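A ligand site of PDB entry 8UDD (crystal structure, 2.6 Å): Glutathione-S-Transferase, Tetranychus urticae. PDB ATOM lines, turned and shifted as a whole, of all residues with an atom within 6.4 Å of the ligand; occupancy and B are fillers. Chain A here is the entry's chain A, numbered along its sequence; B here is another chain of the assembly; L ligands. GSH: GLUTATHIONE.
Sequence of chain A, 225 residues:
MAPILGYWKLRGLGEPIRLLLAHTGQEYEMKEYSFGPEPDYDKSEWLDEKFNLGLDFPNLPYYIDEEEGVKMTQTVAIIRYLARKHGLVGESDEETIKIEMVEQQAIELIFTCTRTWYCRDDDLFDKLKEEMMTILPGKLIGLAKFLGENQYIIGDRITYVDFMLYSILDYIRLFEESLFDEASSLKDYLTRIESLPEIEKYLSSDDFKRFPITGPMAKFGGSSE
Merely in contact with the ligand: Pro 61 (3.2 Å) and Leu 13 (3.7 Å).
Hydrophobic or aromatic side chains that line the ligand: Trp 8, Leu 13, Trp 46 and Pro 61.
Within 4 Å of the ligand: Tyr 7, Trp 8, Leu 13, Trp 46, Lys 50, Asn 59, Leu 60, Pro 61, Gln 74, Thr 75 and Glu 108 of chain B.
The side-chain hydroxyl (OH) of Tyr 7 lies within hydrogen-bond range of the backbone NH (N) of Leu 13, 3.0 Å away.
The side-chain amide nitrogen (NE2) of Gln 105 of chain B is in hydrogen-bond range of the side-chain carboxylate (OE1) of Glu 108 of chain B (3.5 Å).
SG2 of the ligand lies close to OH of Tyr 7, 3.7 Å away.
OE1 of Gln 74 sits at hydrogen-bond distance from N1 of the ligand (2.9 Å).
An oxygen (O32) of the ligand is in salt-bridge range of the side-chain amino group of Lys 50, at 3.4 Å.
The indole nitrogen (NE1) of Trp 46 is in hydrogen-bond range of an oxygen (O32) of the ligand (3.0 Å).
O11 of the ligand sits close to N of Gln 74, at 3.4 Å.
A nitrogen (N2) of the ligand lies within hydrogen-bond range of the backbone carbonyl oxygen of Leu 60, 2.7 Å away.
O12 of the ligand is in hydrogen-bond range of OG1 of Thr 75, 2.7 Å away.
The side-chain carboxylate (OE2) of Glu 108 of chain B lies within salt-bridge range of a nitrogen (N1) of the ligand (2.8 Å).
The backbone NH (N) of Thr 75 is in hydrogen-bond range of an oxygen (O11) of the ligand, 3.0 Å away.
The indole nitrogen (NE1) of Trp 8 sits at hydrogen-bond distance from an oxygen (O2) of the ligand.
OD1 of Asn 59 is in hydrogen-bond range of N3 of the ligand (3.0 Å).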
ATOM      1  N   TYR A   7      24.835 -22.384  19.600  1.00  0.00           N
ATOM      2  CA  TYR A   7      24.482 -21.495  18.483  1.00  0.00           C
ATOM      3  C   TYR A   7      25.441 -21.682  17.307  1.00  0.00           C
ATOM      4  O   TYR A   7      26.441 -22.392  17.430  1.00  0.00           O
ATOM      5  CB  TYR A   7      24.435 -20.018  18.907  1.00  0.00           C
ATOM      6  CG  TYR A   7      23.762 -19.089  17.920  1.00  0.00           C
ATOM      7  CD1 TYR A   7      22.471 -19.309  17.485  1.00  0.00           C
ATOM      8  CD2 TYR A   7      24.438 -18.020  17.355  1.00  0.00           C
ATOM      9  CE1 TYR A   7      21.861 -18.491  16.539  1.00  0.00           C
ATOM     10  CE2 TYR A   7      23.833 -17.160  16.437  1.00  0.00           C
ATOM     11  CZ  TYR A   7      22.535 -17.400  16.027  1.00  0.00           C
ATOM     12  OH  TYR A   7      21.913 -16.573  15.109  1.00  0.00           O
ATOM     13  N   TRP A   8      25.089 -21.066  16.175  1.00  0.00           N
ATOM     14  CA  TRP A   8      26.020 -20.914  15.075  1.00  0.00           C
ATOM     15  C   TRP A   8      27.236 -20.057  15.482  1.00  0.00           C
ATOM     16  O   TRP A   8      27.198 -19.327  16.473  1.00  0.00           O
ATOM     17  CB  TRP A   8      25.309 -20.293  13.873  1.00  0.00           C
ATOM     18  CG  TRP A   8      24.255 -21.172  13.275  1.00  0.00           C
ATOM     19  CD1 TRP A   8      22.933 -20.865  13.182  1.00  0.00           C
ATOM     20  CD2 TRP A   8      24.418 -22.460  12.655  1.00  0.00           C
ATOM     21  NE1 TRP A   8      22.266 -21.885  12.549  1.00  0.00           N
ATOM     22  CE2 TRP A   8      23.143 -22.882  12.228  1.00  0.00           C
ATOM     23  CE3 TRP A   8      25.509 -23.317  12.437  1.00  0.00           C
ATOM     24  CZ2 TRP A   8      22.917 -24.119  11.611  1.00  0.00           C
ATOM     25  CZ3 TRP A   8      25.293 -24.533  11.824  1.00  0.00           C
ATOM     26  CH2 TRP A   8      24.015 -24.932  11.407  1.00  0.00           C
ATOM     27  N   LEU A  10      28.198 -17.202  14.537  1.00  0.00           N
ATOM     28  CA  LEU A  10      27.802 -15.893  13.965  1.00  0.00           C
ATOM     29  C   LEU A  10      27.362 -15.048  15.160  1.00  0.00           C
ATOM     30  O   LEU A  10      27.008 -15.648  16.187  1.00  0.00           O
ATOM     31  CB  LEU A  10      26.618 -16.062  13.005  1.00  0.00           C
ATOM     32  CG  LEU A  10      26.658 -17.226  12.023  1.00  0.00           C
ATOM     33  CD1 LEU A  10      25.262 -17.535  11.502  1.00  0.00           C
ATOM     34  CD2 LEU A  10      27.587 -16.937  10.859  1.00  0.00           C
ATOM     35  N   GLY A  12      24.633 -12.901  15.086  1.00  0.00           N
ATOM     36  CA  GLY A  12      23.190 -13.171  14.973  1.00  0.00           C
ATOM     37  C   GLY A  12      22.346 -12.945  16.210  1.00  0.00           C
ATOM     38  O   GLY A  12      22.410 -11.837  16.777  1.00  0.00           O
ATOM     39  N   LEU A  13      21.563 -13.957  16.604  1.00  0.00           N
ATOM     40  CA  LEU A  13      20.602 -13.810  17.681  1.00  0.00           C
ATOM     41  C   LEU A  13      21.248 -14.193  18.999  1.00  0.00           C
ATOM     42  O   LEU A  13      20.748 -13.841  20.064  1.00  0.00           O
ATOM     43  CB  LEU A  13      19.388 -14.708  17.407  1.00  0.00           C
ATOM     44  CG  LEU A  13      18.612 -14.420  16.121  1.00  0.00           C
ATOM     45  CD1 LEU A  13      17.506 -15.446  15.888  1.00  0.00           C
ATOM     46  CD2 LEU A  13      18.041 -13.016  16.172  1.00  0.00           C
ATOM     47  N   PHE A  35      29.006 -24.004   9.839  1.00  0.00           N
ATOM     48  CA  PHE A  35      28.411 -24.375   8.525  1.00  0.00           C
ATOM     49  C   PHE A  35      29.458 -25.190   7.749  1.00  0.00           C
ATOM     50  O   PHE A  35      30.645 -25.164   8.137  1.00  0.00           O
ATOM     51  CB  PHE A  35      27.985 -23.136   7.745  1.00  0.00           C
ATOM     52  CG  PHE A  35      26.930 -22.274   8.395  1.00  0.00           C
ATOM     53  CD1 PHE A  35      27.211 -21.557   9.549  1.00  0.00           C
ATOM     54  CD2 PHE A  35      25.650 -22.196   7.865  1.00  0.00           C
ATOM     55  CE1 PHE A  35      26.244 -20.767  10.141  1.00  0.00           C
ATOM     56  CE2 PHE A  35      24.686 -21.413   8.464  1.00  0.00           C
ATOM     57  CZ  PHE A  35      24.981 -20.695   9.599  1.00  0.00           C
ATOM     58  N   LYS A  43      24.282 -27.754   7.268  1.00  0.00           N
ATOM     59  CA  LYS A  43      24.039 -27.612   8.722  1.00  0.00           C
ATOM     60  C   LYS A  43      24.278 -28.969   9.385  1.00  0.00           C
ATOM     61  O   LYS A  43      23.771 -29.177  10.494  1.00  0.00           O
ATOM     62  CB  LYS A  43      22.605 -27.139   8.968  1.00  0.00           C
ATOM     63  N   TRP A  46      24.851 -29.414  12.950  1.00  0.00           N
ATOM     64  CA  TRP A  46      23.652 -29.126  13.720  1.00  0.00           C
ATOM     65  C   TRP A  46      22.597 -30.213  13.511  1.00  0.00           C
ATOM     66  O   TRP A  46      22.053 -30.755  14.468  1.00  0.00           O
ATOM     67  CB  TRP A  46      23.130 -27.721  13.361  1.00  0.00           C
ATOM     68  CG  TRP A  46      21.718 -27.408  13.787  1.00  0.00           C
ATOM     69  CD1 TRP A  46      20.727 -26.899  13.001  1.00  0.00           C
ATOM     70  CD2 TRP A  46      21.148 -27.566  15.100  1.00  0.00           C
ATOM     71  NE1 TRP A  46      19.573 -26.740  13.729  1.00  0.00           N
ATOM     72  CE2 TRP A  46      19.806 -27.141  15.017  1.00  0.00           C
ATOM     73  CE3 TRP A  46      21.645 -28.022  16.334  1.00  0.00           C
ATOM     74  CZ2 TRP A  46      18.957 -27.151  16.132  1.00  0.00           C
ATOM     75  CZ3 TRP A  46      20.807 -28.041  17.421  1.00  0.00           C
ATOM     76  CH2 TRP A  46      19.474 -27.604  17.319  1.00  0.00           C
ATOM     77  N   LEU A  47      22.299 -30.535  12.254  1.00  0.00           N
ATOM     78  CA  LEU A  47      21.212 -31.443  11.914  1.00  0.00           C
ATOM     79  C   LEU A  47      21.418 -32.849  12.479  1.00  0.00           C
ATOM     80  O   LEU A  47      20.457 -33.553  12.761  1.00  0.00           O
ATOM     81  CB  LEU A  47      21.049 -31.452  10.390  1.00  0.00           C
ATOM     82  CG  LEU A  47      20.509 -30.149   9.800  1.00  0.00           C
ATOM     83  CD1 LEU A  47      20.337 -30.252   8.286  1.00  0.00           C
ATOM     84  CD2 LEU A  47      19.191 -29.724  10.457  1.00  0.00           C
ATOM     85  N   LYS A  50      20.442 -32.156  16.228  1.00  0.00           N
ATOM     86  CA  LYS A  50      19.267 -31.346  16.469  1.00  0.00           C
ATOM     87  C   LYS A  50      18.219 -32.107  17.307  1.00  0.00           C
ATOM     88  O   LYS A  50      17.650 -31.564  18.266  1.00  0.00           O
ATOM     89  CB  LYS A  50      18.745 -30.933  15.096  1.00  0.00           C
ATOM     90  CG  LYS A  50      17.406 -30.234  15.102  1.00  0.00           C
ATOM     91  CD  LYS A  50      16.906 -29.817  13.726  1.00  0.00           C
ATOM     92  CE  LYS A  50      15.673 -28.932  13.843  1.00  0.00           C
ATOM     93  NZ  LYS A  50      15.419 -28.188  12.590  1.00  0.00           N
ATOM     94  N   PRO A  58      13.311 -28.002  18.577  1.00  0.00           N
ATOM     95  CA  PRO A  58      14.724 -27.944  18.222  1.00  0.00           C
ATOM     96  C   PRO A  58      15.035 -26.740  17.312  1.00  0.00           C
ATOM     97  O   PRO A  58      14.476 -26.683  16.233  1.00  0.00           O
ATOM     98  CB  PRO A  58      14.926 -29.265  17.467  1.00  0.00           C
ATOM     99  CG  PRO A  58      13.944 -30.197  18.124  1.00  0.00           C
ATOM    100  CD  PRO A  58      12.744 -29.337  18.410  1.00  0.00           C
ATOM    101  N   ASN A  59      15.897 -25.836  17.779  1.00  0.00           N
ATOM    102  CA  ASN A  59      16.303 -24.670  16.947  1.00  0.00           C
ATOM    103  C   ASN A  59      17.578 -24.066  17.545  1.00  0.00           C
ATOM    104  O   ASN A  59      17.894 -24.395  18.703  1.00  0.00           O
ATOM    105  CB  ASN A  59      15.206 -23.618  16.838  1.00  0.00           C
ATOM    106  CG  ASN A  59      15.336 -22.767  15.584  1.00  0.00           C
ATOM    107  OD1 ASN A  59      16.391 -22.221  15.315  1.00  0.00           O
ATOM    108  ND2 ASN A  59      14.265 -22.691  14.808  1.00  0.00           N
ATOM    109  N   LEU A  60      18.283 -23.237  16.770  1.00  0.00           N
ATOM    110  CA  LEU A  60      19.485 -22.535  17.302  1.00  0.00           C
ATOM    111  C   LEU A  60      19.169 -21.039  17.392  1.00  0.00           C
ATOM    112  O   LEU A  60      18.836 -20.454  16.353  1.00  0.00           O
ATOM    113  CB  LEU A  60      20.662 -22.791  16.350  1.00  0.00           C
ATOM    114  CG  LEU A  60      21.400 -24.115  16.547  1.00  0.00           C
ATOM    115  CD1 LEU A  60      22.673 -24.151  15.716  1.00  0.00           C
ATOM    116  CD2 LEU A  60      21.730 -24.329  18.024  1.00  0.00           C
ATOM    117  N   PRO A  61      19.232 -20.410  18.585  1.00  0.00           N
ATOM    118  CA  PRO A  61      20.062 -20.907  19.684  1.00  0.00           C
ATOM    119  C   PRO A  61      19.325 -21.830  20.666  1.00  0.00           C
ATOM    120  O   PRO A  61      18.117 -21.881  20.625  1.00  0.00           O
ATOM    121  CB  PRO A  61      20.408 -19.597  20.410  1.00  0.00           C
ATOM    122  CG  PRO A  61      19.161 -18.764  20.258  1.00  0.00           C
ATOM    123  CD  PRO A  61      18.578 -19.144  18.917  1.00  0.00           C
ATOM    124  N   THR A  73      14.627 -23.320  24.085  1.00  0.00           N
ATOM    125  CA  THR A  73      14.949 -22.782  22.742  1.00  0.00           C
ATOM    126  C   THR A  73      14.265 -21.415  22.718  1.00  0.00           C
ATOM    127  O   THR A  73      13.741 -21.018  23.777  1.00  0.00           O
ATOM    128  CB  THR A  73      14.483 -23.698  21.606  1.00  0.00           C
ATOM    129  OG1 THR A  73      13.131 -24.085  21.871  1.00  0.00           O
ATOM    130  CG2 THR A  73      15.351 -24.921  21.454  1.00  0.00           C
ATOM    131  N   GLN A  74      14.282 -20.708  21.587  1.00  0.00           N
ATOM    132  CA  GLN A  74      13.642 -19.371  21.445  1.00  0.00           C
ATOM    133  C   GLN A  74      14.519 -18.309  22.127  1.00  0.00           C
ATOM    134  O   GLN A  74      14.533 -18.273  23.375  1.00  0.00           O
ATOM    135  CB  GLN A  74      12.188 -19.397  21.949  1.00  0.00           C
ATOM    136  CG  GLN A  74      11.335 -20.471  21.292  1.00  0.00           C
ATOM    137  CD  GLN A  74      11.393 -20.422  19.785  1.00  0.00           C
ATOM    138  OE1 GLN A  74      11.064 -19.423  19.153  1.00  0.00           O
ATOM    139  NE2 GLN A  74      11.826 -21.531  19.187  1.00  0.00           N
ATOM    140  N   THR A  75      15.182 -17.463  21.340  1.00  0.00           N
ATOM    141  CA  THR A  75      16.123 -16.436  21.877  1.00  0.00           C
ATOM    142  C   THR A  75      15.456 -15.569  22.949  1.00  0.00           C
ATOM    143  O   THR A  75      16.056 -15.425  24.028  1.00  0.00           O
ATOM    144  CB  THR A  75      16.588 -15.523  20.738  1.00  0.00           C
ATOM    145  OG1 THR A  75      17.053 -16.339  19.666  1.00  0.00           O
ATOM    146  CG2 THR A  75      17.668 -14.555  21.170  1.00  0.00           C
ATOM    147  N   VAL A  76      14.285 -15.007  22.657  1.00  0.00           N
ATOM    148  CA  VAL A  76      13.610 -14.078  23.619  1.00  0.00           C
ATOM    149  C   VAL A  76      13.331 -14.827  24.924  1.00  0.00           C
ATOM    150  O   VAL A  76      13.548 -14.232  25.988  1.00  0.00           O
ATOM    151  CB  VAL A  76      12.323 -13.502  22.999  1.00  0.00           C
ATOM    152  CG1 VAL A  76      11.707 -12.434  23.878  1.00  0.00           C
ATOM    153  CG2 VAL A  76      12.576 -12.984  21.599  1.00  0.00           C
ATOM    154  N   ILE A  78      14.950 -17.409  26.085  1.00  0.00           N
ATOM    155  CA  ILE A  78      16.197 -17.758  26.745  1.00  0.00           C
ATOM    156  C   ILE A  78      16.727 -16.533  27.486  1.00  0.00           C
ATOM    157  O   ILE A  78      17.101 -16.628  28.645  1.00  0.00           O
ATOM    158  CB  ILE A  78      17.240 -18.306  25.760  1.00  0.00           C
ATOM    159  CG1 ILE A  78      16.811 -19.638  25.140  1.00  0.00           C
ATOM    160  CG2 ILE A  78      18.584 -18.440  26.446  1.00  0.00           C
ATOM    161  CD1 ILE A  78      17.775 -20.172  24.106  1.00  0.00           C
ATOM    162  N   TYR A 118      19.147 -11.229   4.377  1.00  0.00           N
ATOM    163  CA  TYR A 118      19.132 -12.652   3.941  1.00  0.00           C
ATOM    164  C   TYR A 118      18.474 -12.798   2.569  1.00  0.00           C
ATOM    165  O   TYR A 118      18.473 -13.928   2.032  1.00  0.00           O
ATOM    166  CB  TYR A 118      18.421 -13.521   4.985  1.00  0.00           C
ATOM    167  CG  TYR A 118      19.320 -14.141   6.024  1.00  0.00           C
ATOM    168  CD1 TYR A 118      20.127 -15.225   5.710  1.00  0.00           C
ATOM    169  CD2 TYR A 118      19.373 -13.639   7.309  1.00  0.00           C
ATOM    170  CE1 TYR A 118      20.963 -15.797   6.657  1.00  0.00           C
ATOM    171  CE2 TYR A 118      20.201 -14.200   8.270  1.00  0.00           C
ATOM    172  CZ  TYR A 118      20.996 -15.283   7.948  1.00  0.00           C
ATOM    173  OH  TYR A 118      21.822 -15.852   8.886  1.00  0.00           O
ATOM    174  N   GLN B 104       6.907 -17.512  21.456  1.00  0.00           N
ATOM    175  CA  GLN B 104       7.876 -17.163  20.428  1.00  0.00           C
ATOM    176  C   GLN B 104       7.691 -18.102  19.237  1.00  0.00           C
ATOM    177  O   GLN B 104       7.774 -17.698  18.084  1.00  0.00           O
ATOM    178  CB  GLN B 104       9.295 -17.214  21.000  1.00  0.00           C
ATOM    179  CG  GLN B 104       9.565 -16.080  21.967  1.00  0.00           C
ATOM    180  CD  GLN B 104       9.419 -14.759  21.238  1.00  0.00           C
ATOM    181  OE1 GLN B 104      10.082 -14.498  20.233  1.00  0.00           O
ATOM    182  NE2 GLN B 104       8.519 -13.914  21.718  1.00  0.00           N
ATOM    183  N   GLN B 105       7.406 -19.362  19.524  1.00  0.00           N
ATOM    184  CA  GLN B 105       7.045 -20.294  18.470  1.00  0.00           C
ATOM    185  C   GLN B 105       5.812 -19.775  17.701  1.00  0.00           C
ATOM    186  O   GLN B 105       5.785 -19.842  16.483  1.00  0.00           O
ATOM    187  CB  GLN B 105       6.883 -21.694  19.058  1.00  0.00           C
ATOM    188  CG  GLN B 105       6.553 -22.722  17.998  1.00  0.00           C
ATOM    189  CD  GLN B 105       7.727 -22.973  17.098  1.00  0.00           C
ATOM    190  OE1 GLN B 105       8.560 -23.826  17.377  1.00  0.00           O
ATOM    191  NE2 GLN B 105       7.751 -22.279  15.966  1.00  0.00           N
ATOM    192  N   GLU B 108       6.870 -16.853  15.445  1.00  0.00           N
ATOM    193  CA  GLU B 108       7.660 -17.360  14.348  1.00  0.00           C
ATOM    194  C   GLU B 108       6.758 -17.758  13.166  1.00  0.00           C
ATOM    195  O   GLU B 108       7.193 -17.685  12.029  1.00  0.00           O
ATOM    196  CB  GLU B 108       8.540 -18.515  14.833  1.00  0.00           C
ATOM    197  CG  GLU B 108       9.526 -19.053  13.818  1.00  0.00           C
ATOM    198  CD  GLU B 108      10.471 -20.092  14.399  1.00  0.00           C
ATOM    199  OE1 GLU B 108      10.404 -21.277  13.974  1.00  0.00           O
ATOM    200  OE2 GLU B 108      11.260 -19.712  15.307  1.00  0.00           O
HETATM  201  N1  GSH L   1      12.549 -18.021  17.083  1.00  0.00           N
HETATM  202  CA1 GSH L   1      13.840 -18.754  17.015  1.00  0.00           C
HETATM  203  C1  GSH L   1      14.793 -18.205  18.071  1.00  0.00           C
HETATM  204  O11 GSH L   1      15.346 -19.027  18.826  1.00  0.00           O
HETATM  205  O12 GSH L   1      14.944 -16.968  18.113  1.00  0.00           O
HETATM  206  CB1 GSH L   1      14.453 -18.643  15.625  1.00  0.00           C
HETATM  207  CG1 GSH L   1      15.848 -19.246  15.553  1.00  0.00           C
HETATM  208  CD1 GSH L   1      16.463 -19.208  14.176  1.00  0.00           C
HETATM  209  OE1 GSH L   1      15.861 -18.756  13.206  1.00  0.00           O
HETATM  210  N2  GSH L   1      17.700 -19.703  14.075  1.00  0.00           N
HETATM  211  CA2 GSH L   1      18.437 -19.729  12.828  1.00  0.00           C
HETATM  212  C2  GSH L   1      18.823 -21.131  12.370  1.00  0.00           C
HETATM  213  O2  GSH L   1      19.555 -21.261  11.385  1.00  0.00           O
HETATM  214  CB2 GSH L   1      19.671 -18.839  12.881  1.00  0.00           C
HETATM  215  SG2 GSH L   1      19.346 -17.106  12.455  1.00  0.00           S
HETATM  216  N3  GSH L   1      18.308 -22.153  13.033  1.00  0.00           N
HETATM  217  CA3 GSH L   1      17.307 -23.002  12.433  1.00  0.00           C
HETATM  218  C3  GSH L   1      17.735 -24.461  12.374  1.00  0.00           C
HETATM  219  O31 GSH L   1      18.749 -24.722  11.689  1.00  0.00           O
HETATM  220  O32 GSH L   1      17.063 -25.294  13.016  1.00  0.00           O
